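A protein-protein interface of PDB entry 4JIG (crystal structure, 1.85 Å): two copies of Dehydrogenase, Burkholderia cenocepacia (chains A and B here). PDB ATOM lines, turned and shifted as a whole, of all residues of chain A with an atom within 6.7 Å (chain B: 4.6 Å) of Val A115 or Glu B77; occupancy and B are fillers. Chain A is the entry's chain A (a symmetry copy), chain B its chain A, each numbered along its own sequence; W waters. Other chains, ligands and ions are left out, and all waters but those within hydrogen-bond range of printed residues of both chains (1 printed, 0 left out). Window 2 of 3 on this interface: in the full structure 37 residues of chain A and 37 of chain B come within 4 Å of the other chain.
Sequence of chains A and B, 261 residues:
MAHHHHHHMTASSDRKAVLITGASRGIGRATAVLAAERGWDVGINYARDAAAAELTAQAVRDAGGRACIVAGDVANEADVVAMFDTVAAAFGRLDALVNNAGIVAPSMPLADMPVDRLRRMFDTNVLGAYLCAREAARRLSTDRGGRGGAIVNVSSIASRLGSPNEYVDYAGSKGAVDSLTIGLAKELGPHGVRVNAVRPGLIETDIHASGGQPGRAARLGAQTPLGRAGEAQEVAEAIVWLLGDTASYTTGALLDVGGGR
NH2 of Arg A119 is in hydrogen-bond range of O of Ala B75, at 3.3 Å. O of Met A113 is in hydrogen-bond range of NH2 of Arg B134 (2.8 Å).
The guanidinium group (NH1) of Arg B134 is in salt-bridge range of the side-chain carboxylate (OE2) of Glu B77 (2.7 Å). The side-chain sulfur (SD) of Met A113 is in hydrogen-bond range of the guanidinium group (NE) of Arg A117, 3.6 Å away.
Among the printed residues, merely in contact across the chains: Pro A114 with Arg B134 (3.9 Å), Val A115 with Glu B77 (3.6 Å), Val A115 with Leu B131 (3.8 Å), Val A115 with Arg B134 (3.5 Å) and Leu A118 with Leu B131 (3.95 Å).
Val A115 touches just these residues of chain B: Glu B77 (3.6 Å), Leu B131 (3.8 Å) and Arg B134 (3.5 Å). Of the printed residues of chain A, Glu B77 touches Val A115 (3.6 Å). Of the printed residues of chain B, Met A113 touches Arg B134. Of the printed residues of chain A, Leu B131 touches Val A115 (3.8 Å) and Leu A118 (3.95 Å). Of the printed residues of chain A, Ala B75 touches Arg A119 (3.3 Å). Of the printed residues of chain B, Leu A118 touches Leu B131 (3.95 Å). Of the printed residues of chain A, Arg B134 touches Met A113, Pro A114 and Val A115. The nearest residue of chain A that does not touch Glu B77 is Arg A119 (5.0 Å). The nearest printed residue of chain B that does not touch Leu A118 is Arg B134 (4.5 Å).
Of the 8 printed residues of chain A, 5 touch a printed residue of chain B. Hydrophobic or aromatic side chains of chain A within 4 Å of the printed part of chain B: Val A115 and Leu A118. Of the 9 printed residues of chain B, 4 touch a printed residue of chain A.
No position is printed for both chains. Of the 7 pairs that touch across the chains among the printed residues, none has its exchanged pair printed and touching as well.
Water W1 lies within hydrogen-bond range of OE2 of Glu B77 (2.8 Å), N of Val A115 (2.9 Å) and NH2 of Arg B134 (3.2 Å).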
ATOM      1  N   MET A 113     -16.498  11.896  -2.497  1.00  0.00           N
ATOM      2  CA  MET A 113     -16.199  12.147  -1.100  1.00  0.00           C
ATOM      3  C   MET A 113     -17.270  11.542  -0.225  1.00  0.00           C
ATOM      4  O   MET A 113     -18.444  11.735  -0.487  1.00  0.00           O
ATOM      5  CB  MET A 113     -16.116  13.656  -0.783  1.00  0.00           C
ATOM      6  CG  MET A 113     -15.005  14.377  -1.496  1.00  0.00           C
ATOM      7  SD  MET A 113     -15.051  16.141  -1.115  1.00  0.00           S
ATOM      8  CE  MET A 113     -13.728  16.701  -2.167  1.00  0.00           C
ATOM      9  N   PRO A 114     -16.868  10.820   0.825  1.00  0.00           N
ATOM     10  CA  PRO A 114     -17.890  10.295   1.710  1.00  0.00           C
ATOM     11  C   PRO A 114     -18.361  11.359   2.656  1.00  0.00           C
ATOM     12  O   PRO A 114     -17.615  12.306   2.972  1.00  0.00           O
ATOM     13  CB  PRO A 114     -17.181   9.186   2.480  1.00  0.00           C
ATOM     14  CG  PRO A 114     -15.744   9.541   2.410  1.00  0.00           C
ATOM     15  CD  PRO A 114     -15.516  10.451   1.239  1.00  0.00           C
ATOM     16  N   VAL A 115     -19.578  11.173   3.131  1.00  0.00           N
ATOM     17  CA  VAL A 115     -20.192  12.122   4.014  1.00  0.00           C
ATOM     18  C   VAL A 115     -19.422  12.362   5.311  1.00  0.00           C
ATOM     19  O   VAL A 115     -19.396  13.478   5.800  1.00  0.00           O
ATOM     20  CB  VAL A 115     -21.666  11.764   4.309  1.00  0.00           C
ATOM     21  CG1 VAL A 115     -21.826  10.470   5.124  1.00  0.00           C
ATOM     22  CG2 VAL A 115     -22.303  12.922   5.039  1.00  0.00           C
ATOM     23  N   ASP A 116     -18.797  11.320   5.875  1.00  0.00           N
ATOM     24  CA  ASP A 116     -18.008  11.512   7.096  1.00  0.00           C
ATOM     25  C   ASP A 116     -16.838  12.498   6.896  1.00  0.00           C
ATOM     26  O   ASP A 116     -16.499  13.287   7.807  1.00  0.00           O
ATOM     27  CB  ASP A 116     -17.448  10.187   7.643  1.00  0.00           C
ATOM     28  N   ARG A 117     -16.206  12.436   5.732  1.00  0.00           N
ATOM     29  CA  ARG A 117     -15.131  13.373   5.415  1.00  0.00           C
ATOM     30  C   ARG A 117     -15.686  14.817   5.298  1.00  0.00           C
ATOM     31  O   ARG A 117     -15.072  15.765   5.796  1.00  0.00           O
ATOM     32  CB  ARG A 117     -14.429  12.949   4.129  1.00  0.00           C
ATOM     33  CG  ARG A 117     -13.391  13.908   3.608  1.00  0.00           C
ATOM     34  CD  ARG A 117     -13.832  14.485   2.290  1.00  0.00           C
ATOM     35  NE  ARG A 117     -12.982  15.544   1.725  1.00  0.00           N
ATOM     36  CZ  ARG A 117     -11.942  15.343   0.916  1.00  0.00           C
ATOM     37  NH1 ARG A 117     -11.544  14.102   0.619  1.00  0.00           N
ATOM     38  NH2 ARG A 117     -11.292  16.392   0.391  1.00  0.00           N
ATOM     39  N   LEU A 118     -16.810  14.967   4.619  1.00  0.00           N
ATOM     40  CA  LEU A 118     -17.430  16.285   4.479  1.00  0.00           C
ATOM     41  C   LEU A 118     -17.742  16.899   5.819  1.00  0.00           C
ATOM     42  O   LEU A 118     -17.395  18.035   6.068  1.00  0.00           O
ATOM     43  CB  LEU A 118     -18.713  16.198   3.670  1.00  0.00           C
ATOM     44  CG  LEU A 118     -18.547  15.904   2.193  1.00  0.00           C
ATOM     45  CD1 LEU A 118     -19.873  15.653   1.474  1.00  0.00           C
ATOM     46  CD2 LEU A 118     -17.783  17.039   1.505  1.00  0.00           C
ATOM     47  N   ARG A 119     -18.356  16.114   6.700  1.00  0.00           N
ATOM     48  CA  ARG A 119     -18.691  16.568   8.040  1.00  0.00           C
ATOM     49  C   ARG A 119     -17.467  16.969   8.816  1.00  0.00           C
ATOM     50  O   ARG A 119     -17.493  17.997   9.492  1.00  0.00           O
ATOM     51  CB  ARG A 119     -19.399  15.473   8.847  1.00  0.00           C
ATOM     52  CG  ARG A 119     -20.857  15.258   8.476  1.00  0.00           C
ATOM     53  CD  ARG A 119     -21.539  14.214   9.400  1.00  0.00           C
ATOM     54  NE  ARG A 119     -22.837  13.864   8.823  1.00  0.00           N
ATOM     55  CZ  ARG A 119     -23.975  14.542   9.006  1.00  0.00           C
ATOM     56  NH1 ARG A 119     -24.030  15.597   9.821  1.00  0.00           N
ATOM     57  NH2 ARG A 119     -25.084  14.153   8.375  1.00  0.00           N
ATOM     58  N   ARG A 120     -16.395  16.172   8.751  1.00  0.00           N
ATOM     59  CA  ARG A 120     -15.182  16.527   9.478  1.00  0.00           C
ATOM     60  C   ARG A 120     -14.579  17.855   8.954  1.00  0.00           C
ATOM     61  O   ARG A 120     -14.022  18.662   9.716  1.00  0.00           O
ATOM     62  CB  ARG A 120     -14.109  15.420   9.419  1.00  0.00           C
ATOM     63  CG  ARG A 120     -14.377  14.209  10.320  1.00  0.00           C
ATOM     64  CD  ARG A 120     -13.227  13.177  10.301  1.00  0.00           C
ATOM     65  NE  ARG A 120     -12.981  12.638   8.965  1.00  0.00           N
ATOM     66  CZ  ARG A 120     -11.856  12.782   8.252  1.00  0.00           C
ATOM     67  NH1 ARG A 120     -10.788  13.404   8.747  1.00  0.00           N
ATOM     68  NH2 ARG A 120     -11.790  12.266   7.024  1.00  0.00           N
ATOM     69  N   ALA B  75     -29.432  18.227   4.899  1.00  0.00           N
ATOM     70  CA  ALA B  75     -28.304  17.834   5.711  1.00  0.00           C
ATOM     71  C   ALA B  75     -28.194  16.320   5.985  1.00  0.00           C
ATOM     72  O   ALA B  75     -27.203  15.846   6.580  1.00  0.00           O
ATOM     73  CB  ALA B  75     -28.361  18.623   7.038  1.00  0.00           C
ATOM     74  N   ASN B  76     -29.185  15.552   5.535  1.00  0.00           N
ATOM     75  CA  ASN B  76     -29.249  14.120   5.860  1.00  0.00           C
ATOM     76  C   ASN B  76     -28.990  13.342   4.571  1.00  0.00           C
ATOM     77  O   ASN B  76     -29.782  13.435   3.642  1.00  0.00           O
ATOM     78  CB  ASN B  76     -30.634  13.813   6.434  1.00  0.00           C
ATOM     79  CG  ASN B  76     -30.810  12.345   6.826  1.00  0.00           C
ATOM     80  OD1 ASN B  76     -30.950  11.484   5.987  1.00  0.00           O
ATOM     81  ND2 ASN B  76     -30.795  12.075   8.115  1.00  0.00           N
ATOM     82  N   GLU B  77     -27.900  12.579   4.521  1.00  0.00           N
ATOM     83  CA  GLU B  77     -27.499  11.873   3.329  1.00  0.00           C
ATOM     84  C   GLU B  77     -28.605  10.960   2.760  1.00  0.00           C
ATOM     85  O   GLU B  77     -28.843  10.917   1.543  1.00  0.00           O
ATOM     86  CB  GLU B  77     -26.302  10.992   3.632  1.00  0.00           C
ATOM     87  CG  GLU B  77     -25.917  10.188   2.447  1.00  0.00           C
ATOM     88  CD  GLU B  77     -24.647   9.419   2.643  1.00  0.00           C
ATOM     89  OE1 GLU B  77     -24.523   8.688   3.643  1.00  0.00           O
ATOM     90  OE2 GLU B  77     -23.790   9.533   1.754  1.00  0.00           O
ATOM     91  N   ALA B  78     -29.250  10.201   3.656  1.00  0.00           N
ATOM     92  CA  ALA B  78     -30.303   9.300   3.215  1.00  0.00           C
ATOM     93  C   ALA B  78     -31.467  10.084   2.584  1.00  0.00           C
ATOM     94  O   ALA B  78     -31.945   9.673   1.533  1.00  0.00           O
ATOM     95  CB  ALA B  78     -30.766   8.400   4.363  1.00  0.00           C
ATOM     96  N   ASP B  79     -31.892  11.205   3.188  1.00  0.00           N
ATOM     97  CA  ASP B  79     -32.944  12.038   2.594  1.00  0.00           C
ATOM     98  C   ASP B  79     -32.545  12.565   1.197  1.00  0.00           C
ATOM     99  O   ASP B  79     -33.362  12.625   0.269  1.00  0.00           O
ATOM    100  CB  ASP B  79     -33.309  13.265   3.479  1.00  0.00           C
ATOM    101  CG  ASP B  79     -34.087  12.915   4.752  1.00  0.00           C
ATOM    102  OD1 ASP B  79     -34.390  11.729   5.009  1.00  0.00           O
ATOM    103  OD2 ASP B  79     -34.408  13.867   5.500  1.00  0.00           O
ATOM    104  N   VAL B  80     -31.298  12.993   1.057  1.00  0.00           N
ATOM    105  CA  VAL B  80     -30.822  13.554  -0.210  1.00  0.00           C
ATOM    106  C   VAL B  80     -30.824  12.481  -1.313  1.00  0.00           C
ATOM    107  O   VAL B  80     -31.283  12.734  -2.408  1.00  0.00           O
ATOM    108  CB  VAL B  80     -29.422  14.198  -0.051  1.00  0.00           C
ATOM    109  CG1 VAL B  80     -28.812  14.555  -1.402  1.00  0.00           C
ATOM    110  CG2 VAL B  80     -29.523  15.402   0.839  1.00  0.00           C
ATOM    111  N   VAL B  81     -30.292  11.305  -1.028  1.00  0.00           N
ATOM    112  CA  VAL B  81     -30.295  10.204  -2.009  1.00  0.00           C
ATOM    113  C   VAL B  81     -31.757   9.867  -2.389  1.00  0.00           C
ATOM    114  O   VAL B  81     -32.049   9.704  -3.572  1.00  0.00           O
ATOM    115  CB  VAL B  81     -29.511   8.960  -1.533  1.00  0.00           C
ATOM    116  CG1 VAL B  81     -29.725   7.772  -2.485  1.00  0.00           C
ATOM    117  CG2 VAL B  81     -28.010   9.281  -1.418  1.00  0.00           C
ATOM    118  N   LEU B 131     -24.059  18.109  -0.077  1.00  0.00           N
ATOM    119  CA  LEU B 131     -24.638  16.775  -0.333  1.00  0.00           C
ATOM    120  C   LEU B 131     -25.514  16.766  -1.585  1.00  0.00           C
ATOM    121  O   LEU B 131     -25.520  15.799  -2.383  1.00  0.00           O
ATOM    122  CB  LEU B 131     -25.391  16.272   0.890  1.00  0.00           C
ATOM    123  CG  LEU B 131     -24.567  15.893   2.143  1.00  0.00           C
ATOM    124  CD1 LEU B 131     -25.486  15.668   3.340  1.00  0.00           C
ATOM    125  CD2 LEU B 131     -23.674  14.671   1.913  1.00  0.00           C
ATOM    126  N   ARG B 134     -23.223  17.123  -4.553  1.00  0.00           N
ATOM    127  CA  ARG B 134     -22.544  15.833  -4.718  1.00  0.00           C
ATOM    128  C   ARG B 134     -23.443  14.845  -5.479  1.00  0.00           C
ATOM    129  O   ARG B 134     -22.990  14.096  -6.368  1.00  0.00           O
ATOM    130  CB  ARG B 134     -22.134  15.250  -3.359  1.00  0.00           C
ATOM    131  CG  ARG B 134     -21.422  13.906  -3.490  1.00  0.00           C
ATOM    132  CD  ARG B 134     -21.044  13.274  -2.155  1.00  0.00           C
ATOM    133  NE  ARG B 134     -22.243  12.726  -1.549  1.00  0.00           N
ATOM    134  CZ  ARG B 134     -22.308  11.863  -0.548  1.00  0.00           C
ATOM    135  NH1 ARG B 134     -23.516  11.493  -0.126  1.00  0.00           N
ATOM    136  NH2 ARG B 134     -21.212  11.367   0.024  1.00  0.00           N
HETATM  137  O   HOH W   1     -21.040   8.883   1.985  1.00  0.00           O
